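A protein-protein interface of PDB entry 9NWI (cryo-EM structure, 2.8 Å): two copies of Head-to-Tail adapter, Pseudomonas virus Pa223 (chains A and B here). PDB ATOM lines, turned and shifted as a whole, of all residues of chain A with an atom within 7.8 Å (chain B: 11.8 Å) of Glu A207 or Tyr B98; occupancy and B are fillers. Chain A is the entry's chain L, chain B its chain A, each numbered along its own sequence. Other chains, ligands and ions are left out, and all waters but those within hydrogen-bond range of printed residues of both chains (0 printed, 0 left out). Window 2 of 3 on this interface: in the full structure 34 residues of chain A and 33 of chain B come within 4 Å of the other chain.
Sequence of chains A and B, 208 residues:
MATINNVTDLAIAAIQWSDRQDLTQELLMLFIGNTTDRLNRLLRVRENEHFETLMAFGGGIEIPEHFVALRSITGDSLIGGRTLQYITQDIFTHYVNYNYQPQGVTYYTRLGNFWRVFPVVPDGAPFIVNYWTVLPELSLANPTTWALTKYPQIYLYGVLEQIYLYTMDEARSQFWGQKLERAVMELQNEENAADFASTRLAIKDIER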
ATOM      1  N   ARG A  82       5.679  -7.234  -4.811  1.00  0.00           N
ATOM      2  CA  ARG A  82       5.012  -7.176  -3.520  1.00  0.00           C
ATOM      3  C   ARG A  82       4.339  -5.824  -3.329  1.00  0.00           C
ATOM      4  O   ARG A  82       4.566  -4.874  -4.079  1.00  0.00           O
ATOM      5  CB  ARG A  82       6.010  -7.433  -2.390  1.00  0.00           C
ATOM      6  CG  ARG A  82       6.991  -8.533  -2.705  1.00  0.00           C
ATOM      7  CD  ARG A  82       8.152  -8.518  -1.743  1.00  0.00           C
ATOM      8  NE  ARG A  82       7.786  -9.087  -0.454  1.00  0.00           N
ATOM      9  CZ  ARG A  82       8.356 -10.161   0.069  1.00  0.00           C
ATOM     10  NH1 ARG A  82       9.304 -10.821  -0.577  1.00  0.00           N
ATOM     11  NH2 ARG A  82       7.963 -10.589   1.265  1.00  0.00           N
ATOM     12  N   GLN A 103      14.491 -10.189   1.166  1.00  0.00           N
ATOM     13  CA  GLN A 103      14.580 -10.794  -0.157  1.00  0.00           C
ATOM     14  C   GLN A 103      14.001  -9.912  -1.257  1.00  0.00           C
ATOM     15  O   GLN A 103      14.445 -10.001  -2.407  1.00  0.00           O
ATOM     16  CB  GLN A 103      13.899 -12.167  -0.156  1.00  0.00           C
ATOM     17  CG  GLN A 103      12.366 -12.219   0.021  1.00  0.00           C
ATOM     18  CD  GLN A 103      11.816 -11.511   1.264  1.00  0.00           C
ATOM     19  OE1 GLN A 103      12.428 -10.603   1.826  1.00  0.00           O
ATOM     20  NE2 GLN A 103      10.648 -11.958   1.712  1.00  0.00           N
ATOM     21  N   TYR A 107       9.317  -2.072   1.889  1.00  0.00           N
ATOM     22  CA  TYR A 107       8.913  -0.914   2.670  1.00  0.00           C
ATOM     23  C   TYR A 107       9.128   0.373   1.888  1.00  0.00           C
ATOM     24  O   TYR A 107       9.923   0.433   0.949  1.00  0.00           O
ATOM     25  CB  TYR A 107       9.683  -0.852   3.992  1.00  0.00           C
ATOM     26  CG  TYR A 107       9.569  -2.112   4.812  1.00  0.00           C
ATOM     27  CD1 TYR A 107       8.393  -2.427   5.474  1.00  0.00           C
ATOM     28  CD2 TYR A 107      10.635  -2.990   4.919  1.00  0.00           C
ATOM     29  CE1 TYR A 107       8.284  -3.577   6.221  1.00  0.00           C
ATOM     30  CE2 TYR A 107      10.534  -4.142   5.666  1.00  0.00           C
ATOM     31  CZ  TYR A 107       9.357  -4.431   6.314  1.00  0.00           C
ATOM     32  OH  TYR A 107       9.251  -5.580   7.059  1.00  0.00           O
ATOM     33  N   LYS A 204      -8.268 -13.339   6.343  1.00  0.00           N
ATOM     34  CA  LYS A 204      -7.210 -14.199   5.837  1.00  0.00           C
ATOM     35  C   LYS A 204      -5.884 -13.839   6.493  1.00  0.00           C
ATOM     36  O   LYS A 204      -5.700 -12.732   7.005  1.00  0.00           O
ATOM     37  CB  LYS A 204      -7.088 -14.092   4.313  1.00  0.00           C
ATOM     38  CG  LYS A 204      -8.419 -14.119   3.591  1.00  0.00           C
ATOM     39  CD  LYS A 204      -9.171 -15.402   3.885  1.00  0.00           C
ATOM     40  CE  LYS A 204     -10.153 -15.733   2.780  1.00  0.00           C
ATOM     41  NZ  LYS A 204     -11.145 -16.749   3.220  1.00  0.00           N
ATOM     42  N   ASP A 205      -4.958 -14.792   6.475  1.00  0.00           N
ATOM     43  CA  ASP A 205      -3.665 -14.652   7.129  1.00  0.00           C
ATOM     44  C   ASP A 205      -2.567 -14.485   6.088  1.00  0.00           C
ATOM     45  O   ASP A 205      -2.518 -15.231   5.106  1.00  0.00           O
ATOM     46  CB  ASP A 205      -3.360 -15.865   8.008  1.00  0.00           C
ATOM     47  CG  ASP A 205      -4.549 -16.297   8.835  1.00  0.00           C
ATOM     48  OD1 ASP A 205      -4.499 -17.402   9.413  1.00  0.00           O
ATOM     49  OD2 ASP A 205      -5.533 -15.534   8.912  1.00  0.00           O
ATOM     50  N   ILE A 206      -1.693 -13.504   6.308  1.00  0.00           N
ATOM     51  CA  ILE A 206      -0.519 -13.286   5.478  1.00  0.00           C
ATOM     52  C   ILE A 206       0.686 -13.139   6.396  1.00  0.00           C
ATOM     53  O   ILE A 206       0.556 -12.870   7.591  1.00  0.00           O
ATOM     54  CB  ILE A 206      -0.658 -12.050   4.567  1.00  0.00           C
ATOM     55  CG1 ILE A 206      -0.739 -10.775   5.405  1.00  0.00           C
ATOM     56  CG2 ILE A 206      -1.882 -12.172   3.683  1.00  0.00           C
ATOM     57  CD1 ILE A 206      -0.274  -9.540   4.675  1.00  0.00           C
ATOM     58  N   GLU A 207       1.874 -13.326   5.822  1.00  0.00           N
ATOM     59  CA  GLU A 207       3.107 -13.263   6.593  1.00  0.00           C
ATOM     60  C   GLU A 207       3.929 -12.010   6.341  1.00  0.00           C
ATOM     61  O   GLU A 207       4.809 -11.704   7.152  1.00  0.00           O
ATOM     62  CB  GLU A 207       3.982 -14.492   6.305  1.00  0.00           C
ATOM     63  CG  GLU A 207       4.899 -14.332   5.107  1.00  0.00           C
ATOM     64  CD  GLU A 207       4.133 -14.158   3.813  1.00  0.00           C
ATOM     65  OE1 GLU A 207       2.980 -14.628   3.744  1.00  0.00           O
ATOM     66  OE2 GLU A 207       4.679 -13.549   2.870  1.00  0.00           O
ATOM     67  N   ARG A 208       3.665 -11.286   5.255  1.00  0.00           N
ATOM     68  CA  ARG A 208       4.402 -10.070   4.897  1.00  0.00           C
ATOM     69  C   ARG A 208       5.893 -10.341   4.701  1.00  0.00           C
ATOM     70  O   ARG A 208       6.663 -10.469   5.651  1.00  0.00           O
ATOM     71  CB  ARG A 208       4.199  -8.981   5.956  1.00  0.00           C
ATOM     72  CG  ARG A 208       5.062  -7.747   5.755  1.00  0.00           C
ATOM     73  CD  ARG A 208       4.490  -6.835   4.685  1.00  0.00           C
ATOM     74  NE  ARG A 208       3.173  -6.326   5.045  1.00  0.00           N
ATOM     75  CZ  ARG A 208       2.272  -5.901   4.172  1.00  0.00           C
ATOM     76  NH1 ARG A 208       2.511  -5.908   2.873  1.00  0.00           N
ATOM     77  NH2 ARG A 208       1.100  -5.455   4.616  1.00  0.00           N
ATOM     78  OXT ARG A 208       6.369 -10.427   3.569  1.00  0.00           O
ATOM     79  N   ILE B  87     -11.239 -10.070  -1.373  1.00  0.00           N
ATOM     80  CA  ILE B  87      -9.971  -9.980  -0.665  1.00  0.00           C
ATOM     81  C   ILE B  87      -9.320  -8.647  -1.000  1.00  0.00           C
ATOM     82  O   ILE B  87      -9.599  -8.033  -2.030  1.00  0.00           O
ATOM     83  CB  ILE B  87      -9.016 -11.140  -1.010  1.00  0.00           C
ATOM     84  CG1 ILE B  87      -8.768 -11.193  -2.515  1.00  0.00           C
ATOM     85  CG2 ILE B  87      -9.577 -12.458  -0.515  1.00  0.00           C
ATOM     86  CD1 ILE B  87      -7.698 -12.176  -2.915  1.00  0.00           C
ATOM     87  N   THR B  88      -8.438  -8.203  -0.111  1.00  0.00           N
ATOM     88  CA  THR B  88      -7.737  -6.946  -0.310  1.00  0.00           C
ATOM     89  C   THR B  88      -6.557  -7.145  -1.259  1.00  0.00           C
ATOM     90  O   THR B  88      -6.242  -8.260  -1.681  1.00  0.00           O
ATOM     91  CB  THR B  88      -7.271  -6.376   1.024  1.00  0.00           C
ATOM     92  OG1 THR B  88      -5.998  -6.937   1.365  1.00  0.00           O
ATOM     93  CG2 THR B  88      -8.269  -6.703   2.117  1.00  0.00           C
ATOM     94  N   GLN B  89      -5.895  -6.040  -1.604  1.00  0.00           N
ATOM     95  CA  GLN B  89      -4.782  -6.108  -2.544  1.00  0.00           C
ATOM     96  C   GLN B  89      -3.599  -6.868  -1.957  1.00  0.00           C
ATOM     97  O   GLN B  89      -2.931  -7.628  -2.668  1.00  0.00           O
ATOM     98  CB  GLN B  89      -4.363  -4.698  -2.958  1.00  0.00           C
ATOM     99  CG  GLN B  89      -3.066  -4.643  -3.738  1.00  0.00           C
ATOM    100  CD  GLN B  89      -3.265  -4.902  -5.214  1.00  0.00           C
ATOM    101  OE1 GLN B  89      -4.360  -5.253  -5.652  1.00  0.00           O
ATOM    102  NE2 GLN B  89      -2.206  -4.730  -5.993  1.00  0.00           N
ATOM    103  N   ASP B  90      -3.319  -6.672  -0.667  1.00  0.00           N
ATOM    104  CA  ASP B  90      -2.185  -7.350  -0.048  1.00  0.00           C
ATOM    105  C   ASP B  90      -2.369  -8.861  -0.057  1.00  0.00           C
ATOM    106  O   ASP B  90      -1.427  -9.607  -0.350  1.00  0.00           O
ATOM    107  CB  ASP B  90      -1.990  -6.846   1.380  1.00  0.00           C
ATOM    108  CG  ASP B  90      -2.073  -5.339   1.478  1.00  0.00           C
ATOM    109  OD1 ASP B  90      -2.997  -4.754   0.876  1.00  0.00           O
ATOM    110  OD2 ASP B  90      -1.212  -4.739   2.154  1.00  0.00           O
ATOM    111  N   ILE B  91      -3.575  -9.330   0.263  1.00  0.00           N
ATOM    112  CA  ILE B  91      -3.842 -10.764   0.241  1.00  0.00           C
ATOM    113  C   ILE B  91      -3.698 -11.308  -1.172  1.00  0.00           C
ATOM    114  O   ILE B  91      -3.149 -12.395  -1.381  1.00  0.00           O
ATOM    115  CB  ILE B  91      -5.236 -11.054   0.824  1.00  0.00           C
ATOM    116  CG1 ILE B  91      -5.333 -10.526   2.253  1.00  0.00           C
ATOM    117  CG2 ILE B  91      -5.525 -12.538   0.793  1.00  0.00           C
ATOM    118  CD1 ILE B  91      -6.736 -10.520   2.802  1.00  0.00           C
ATOM    119  N   PHE B  92      -4.193 -10.564  -2.161  1.00  0.00           N
ATOM    120  CA  PHE B  92      -4.061 -10.981  -3.553  1.00  0.00           C
ATOM    121  C   PHE B  92      -2.596 -11.129  -3.942  1.00  0.00           C
ATOM    122  O   PHE B  92      -2.195 -12.133  -4.543  1.00  0.00           O
ATOM    123  CB  PHE B  92      -4.759  -9.964  -4.455  1.00  0.00           C
ATOM    124  CG  PHE B  92      -4.911 -10.408  -5.879  1.00  0.00           C
ATOM    125  CD1 PHE B  92      -3.870 -10.267  -6.779  1.00  0.00           C
ATOM    126  CD2 PHE B  92      -6.102 -10.945  -6.323  1.00  0.00           C
ATOM    127  CE1 PHE B  92      -4.012 -10.668  -8.087  1.00  0.00           C
ATOM    128  CE2 PHE B  92      -6.248 -11.344  -7.630  1.00  0.00           C
ATOM    129  CZ  PHE B  92      -5.201 -11.208  -8.513  1.00  0.00           C
ATOM    130  N   THR B  93      -1.780 -10.131  -3.602  1.00  0.00           N
ATOM    131  CA  THR B  93      -0.365 -10.179  -3.950  1.00  0.00           C
ATOM    132  C   THR B  93       0.335 -11.336  -3.251  1.00  0.00           C
ATOM    133  O   THR B  93       1.143 -12.044  -3.865  1.00  0.00           O
ATOM    134  CB  THR B  93       0.299  -8.850  -3.597  1.00  0.00           C
ATOM    135  OG1 THR B  93      -0.020  -7.879  -4.599  1.00  0.00           O
ATOM    136  CG2 THR B  93       1.804  -9.006  -3.519  1.00  0.00           C
ATOM    137  N   HIS B  94       0.034 -11.550  -1.969  1.00  0.00           N
ATOM    138  CA  HIS B  94       0.657 -12.652  -1.245  1.00  0.00           C
ATOM    139  C   HIS B  94       0.270 -13.997  -1.847  1.00  0.00           C
ATOM    140  O   HIS B  94       1.118 -14.883  -2.002  1.00  0.00           O
ATOM    141  CB  HIS B  94       0.268 -12.597   0.228  1.00  0.00           C
ATOM    142  CG  HIS B  94       0.681 -13.808   1.003  1.00  0.00           C
ATOM    143  ND1 HIS B  94      -0.170 -14.466   1.864  1.00  0.00           N
ATOM    144  CD2 HIS B  94       1.853 -14.481   1.045  1.00  0.00           C
ATOM    145  CE1 HIS B  94       0.461 -15.494   2.402  1.00  0.00           C
ATOM    146  NE2 HIS B  94       1.691 -15.523   1.924  1.00  0.00           N
ATOM    147  N   TYR B  95      -1.008 -14.165  -2.192  1.00  0.00           N
ATOM    148  CA  TYR B  95      -1.453 -15.415  -2.798  1.00  0.00           C
ATOM    149  C   TYR B  95      -0.774 -15.645  -4.139  1.00  0.00           C
ATOM    150  O   TYR B  95      -0.389 -16.773  -4.462  1.00  0.00           O
ATOM    151  CB  TYR B  95      -2.970 -15.407  -2.963  1.00  0.00           C
ATOM    152  CG  TYR B  95      -3.727 -15.739  -1.704  1.00  0.00           C
ATOM    153  CD1 TYR B  95      -3.063 -16.148  -0.559  1.00  0.00           C
ATOM    154  CD2 TYR B  95      -5.108 -15.641  -1.659  1.00  0.00           C
ATOM    155  CE1 TYR B  95      -3.753 -16.451   0.593  1.00  0.00           C
ATOM    156  CE2 TYR B  95      -5.806 -15.942  -0.512  1.00  0.00           C
ATOM    157  CZ  TYR B  95      -5.124 -16.346   0.611  1.00  0.00           C
ATOM    158  OH  TYR B  95      -5.818 -16.648   1.759  1.00  0.00           O
ATOM    159  N   VAL B  96      -0.628 -14.588  -4.939  1.00  0.00           N
ATOM    160  CA  VAL B  96       0.055 -14.729  -6.221  1.00  0.00           C
ATOM    161  C   VAL B  96       1.507 -15.131  -6.005  1.00  0.00           C
ATOM    162  O   VAL B  96       2.031 -16.017  -6.691  1.00  0.00           O
ATOM    163  CB  VAL B  96      -0.057 -13.426  -7.032  1.00  0.00           C
ATOM    164  CG1 VAL B  96       0.993 -13.391  -8.126  1.00  0.00           C
ATOM    165  CG2 VAL B  96      -1.445 -13.294  -7.623  1.00  0.00           C
ATOM    166  N   ASN B  97       2.176 -14.497  -5.042  1.00  0.00           N
ATOM    167  CA  ASN B  97       3.598 -14.753  -4.838  1.00  0.00           C
ATOM    168  C   ASN B  97       3.848 -16.152  -4.293  1.00  0.00           C
ATOM    169  O   ASN B  97       4.836 -16.797  -4.660  1.00  0.00           O
ATOM    170  CB  ASN B  97       4.186 -13.703  -3.899  1.00  0.00           C
ATOM    171  CG  ASN B  97       4.649 -12.466  -4.631  1.00  0.00           C
ATOM    172  OD1 ASN B  97       4.414 -12.317  -5.829  1.00  0.00           O
ATOM    173  ND2 ASN B  97       5.312 -11.568  -3.915  1.00  0.00           N
ATOM    174  N   TYR B  98       2.976 -16.640  -3.416  1.00  0.00           N
ATOM    175  CA  TYR B  98       3.219 -17.903  -2.731  1.00  0.00           C
ATOM    176  C   TYR B  98       2.617 -19.108  -3.439  1.00  0.00           C
ATOM    177  O   TYR B  98       2.785 -20.231  -2.952  1.00  0.00           O
ATOM    178  CB  TYR B  98       2.682 -17.835  -1.301  1.00  0.00           C
ATOM    179  CG  TYR B  98       3.686 -17.315  -0.303  1.00  0.00           C
ATOM    180  CD1 TYR B  98       4.555 -16.288  -0.636  1.00  0.00           C
ATOM    181  CD2 TYR B  98       3.766 -17.854   0.973  1.00  0.00           C
ATOM    182  CE1 TYR B  98       5.473 -15.809   0.273  1.00  0.00           C
ATOM    183  CE2 TYR B  98       4.682 -17.382   1.888  1.00  0.00           C
ATOM    184  CZ  TYR B  98       5.533 -16.359   1.533  1.00  0.00           C
ATOM    185  OH  TYR B  98       6.448 -15.886   2.444  1.00  0.00           O
ATOM    186  N   ASN B  99       1.923 -18.911  -4.562  1.00  0.00           N
ATOM    187  CA  ASN B  99       1.309 -19.999  -5.324  1.00  0.00           C
ATOM    188  C   ASN B  99       0.342 -20.800  -4.447  1.00  0.00           C
ATOM    189  O   ASN B  99       0.543 -21.980  -4.152  1.00  0.00           O
ATOM    190  CB  ASN B  99       2.377 -20.908  -5.941  1.00  0.00           C
ATOM    191  CG  ASN B  99       2.631 -20.598  -7.397  1.00  0.00           C
ATOM    192  OD1 ASN B  99       1.910 -21.064  -8.277  1.00  0.00           O
ATOM    193  ND2 ASN B  99       3.661 -19.805  -7.661  1.00  0.00           N
ATOM    194  N   TYR B 100      -0.720 -20.110  -4.027  1.00  0.00           N
ATOM    195  CA  TYR B 100      -1.698 -20.721  -3.134  1.00  0.00           C
ATOM    196  C   TYR B 100      -2.361 -21.934  -3.776  1.00  0.00           C
ATOM    197  O   TYR B 100      -2.510 -22.980  -3.133  1.00  0.00           O
ATOM    198  CB  TYR B 100      -2.745 -19.687  -2.729  1.00  0.00           C
ATOM    199  CG  TYR B 100      -3.756 -20.198  -1.735  1.00  0.00           C
ATOM    200  CD1 TYR B 100      -3.371 -20.995  -0.670  1.00  0.00           C
ATOM    201  CD2 TYR B 100      -5.100 -19.884  -1.865  1.00  0.00           C
ATOM    202  CE1 TYR B 100      -4.294 -21.464   0.238  1.00  0.00           C
ATOM    203  CE2 TYR B 100      -6.031 -20.348  -0.963  1.00  0.00           C
ATOM    204  CZ  TYR B 100      -5.624 -21.137   0.087  1.00  0.00           C
ATOM    205  OH  TYR B 100      -6.549 -21.602   0.990  1.00  0.00           O
ATOM    206  N   GLN B 101      -2.758 -21.815  -5.042  1.00  0.00           N
ATOM    207  CA  GLN B 101      -3.336 -22.902  -5.826  1.00  0.00           C
ATOM    208  C   GLN B 101      -4.526 -23.569  -5.142  1.00  0.00           C
ATOM    209  O   GLN B 101      -4.406 -24.704  -4.666  1.00  0.00           O
ATOM    210  CB  GLN B 101      -2.274 -23.957  -6.132  1.00  0.00           C
ATOM    211  CG  GLN B 101      -1.025 -23.404  -6.786  1.00  0.00           C
ATOM    212  CD  GLN B 101      -0.363 -24.407  -7.703  1.00  0.00           C
ATOM    213  OE1 GLN B 101      -0.409 -25.612  -7.459  1.00  0.00           O
ATOM    214  NE2 GLN B 101       0.258 -23.914  -8.768  1.00  0.00           N
ATOM    215  N   PRO B 102      -5.677 -22.913  -5.071  1.00  0.00           N
ATOM    216  CA  PRO B 102      -6.898 -23.588  -4.628  1.00  0.00           C
ATOM    217  C   PRO B 102      -7.494 -24.383  -5.785  1.00  0.00           C
ATOM    218  O   PRO B 102      -6.926 -24.466  -6.871  1.00  0.00           O
ATOM    219  CB  PRO B 102      -7.814 -22.436  -4.196  1.00  0.00           C
ATOM    220  CG  PRO B 102      -7.098 -21.160  -4.571  1.00  0.00           C
ATOM    221  CD  PRO B 102      -5.934 -21.513  -5.434  1.00  0.00           C
ATOM    222  N   PHE B 118      -8.231 -14.247  -8.459  1.00  0.00           N
ATOM    223  CA  PHE B 118      -6.888 -14.701  -8.096  1.00  0.00           C
ATOM    224  C   PHE B 118      -6.422 -15.874  -8.949  1.00  0.00           C
ATOM    225  O   PHE B 118      -5.364 -15.763  -9.592  1.00  0.00           O
ATOM    226  CB  PHE B 118      -6.815 -15.016  -6.601  1.00  0.00           C
ATOM    227  CG  PHE B 118      -5.716 -15.973  -6.252  1.00  0.00           C
ATOM    228  CD1 PHE B 118      -4.396 -15.664  -6.535  1.00  0.00           C
ATOM    229  CD2 PHE B 118      -6.001 -17.189  -5.665  1.00  0.00           C
ATOM    230  CE1 PHE B 118      -3.386 -16.544  -6.232  1.00  0.00           C
ATOM    231  CE2 PHE B 118      -4.991 -18.072  -5.355  1.00  0.00           C
ATOM    232  CZ  PHE B 118      -3.683 -17.749  -5.639  1.00  0.00           C
ATOM    233  N   PRO B 119      -7.124 -17.012  -9.001  1.00  0.00           N
ATOM    234  CA  PRO B 119      -6.631 -18.100  -9.850  1.00  0.00           C
ATOM    235  C   PRO B 119      -6.790 -17.719 -11.308  1.00  0.00           C
ATOM    236  O   PRO B 119      -7.779 -18.082 -11.950  1.00  0.00           O
ATOM    237  CB  PRO B 119      -7.512 -19.293  -9.458  1.00  0.00           C
ATOM    238  CG  PRO B 119      -8.184 -18.884  -8.186  1.00  0.00           C
ATOM    239  CD  PRO B 119      -8.357 -17.413  -8.304  1.00  0.00           C
ATOM    240  N   VAL B 120      -5.819 -16.950 -11.814  1.00  0.00           N
ATOM    241  CA  VAL B 120      -5.929 -16.317 -13.121  1.00  0.00           C
ATOM    242  C   VAL B 120      -6.331 -17.342 -14.164  1.00  0.00           C
ATOM    243  O   VAL B 120      -5.724 -18.412 -14.277  1.00  0.00           O
ATOM    244  CB  VAL B 120      -4.604 -15.630 -13.491  1.00  0.00           C
ATOM    245  CG1 VAL B 120      -4.738 -14.902 -14.816  1.00  0.00           C
ATOM    246  CG2 VAL B 120      -4.183 -14.672 -12.393  1.00  0.00           C
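The side-chain carboxylate of Asp B90 lies within salt-bridge range of the guanidinium group of Arg A208 (3.5 Å). A ring nitrogen (NE2) of His B94 lies within hydrogen-bond range of the side-chain carboxylate (OE1) of Glu A207 (2.4 Å). The side-chain hydroxyl of Tyr B98 lies within hydrogen-bond range of the side-chain carboxylate of Glu A207, at 3.0 Å.
The side-chain hydroxyl of Thr B88 lies close to the backbone NH of Asp B90, at 3.4 Å. The backbone carbonyl oxygen (O) of Tyr B95 lies within hydrogen-bond range of the backbone NH (N) of Tyr B100 (3.4 Å). NH1 of Arg A82 lies close to NE2 of Gln A103 (2.9 Å). OXT of Arg A208 is in salt-bridge range of NH2 of Arg A82, at 2.8 Å.
Among the printed residues, pairs that only touch across the chains: Arg A82 with Thr B93, Arg A82 with Asn B97, Lys A204 with Ile B91, Lys A204 with Tyr B95 and Ile A206 with His B94.
Of chain B, only His B94 (2.4 Å) and Tyr B98 (3.0 Å) come within 4 Å of Glu A207. Tyr B98 touches just one residue of chain A: Glu A207. Arg A208 touches just one residue of chain B: Asp B90. Of the printed residues of chain A, Ile B91 touches Lys A204. Of the printed residues of chain A, His B94 touches Ile A206 (3.4 Å) and Glu A207 (2.4 Å). Of the printed residues of chain B, Arg A82 touches Thr B93 (3.7 Å) and Asn B97 (3.7 Å). Printed residues of chain A within 4 Å of Asn B97: Arg A82. Asp A205 touches none of the printed residues of chain B. The nearest printed residue of chain A that does not touch Asp B90 is Ile A206 (4.6 Å).
Of the 8 printed residues of chain A, 5 touch a printed residue of chain B. Printed residues of chain A that touch a printed residue of chain B: Arg A82, Lys A204, Ile A206, Glu A207 and Arg A208. Of the 19 printed residues of chain B, 7 touch a printed residue of chain A. Hydrophobic or aromatic side chains of chain B that line the printed part of chain A: Ile B91, His B94, Tyr B95 and Tyr B98. Among the printed residues, Asp or Glu carboxylates within 4 Å of a Lys or Arg side-chain nitrogen of the other chain: Arg A208 with Asp B90.
No position is printed for both chains. Of the 8 pairs that touch across the chains among the printed residues, none has its exchanged pair printed and touching as well.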
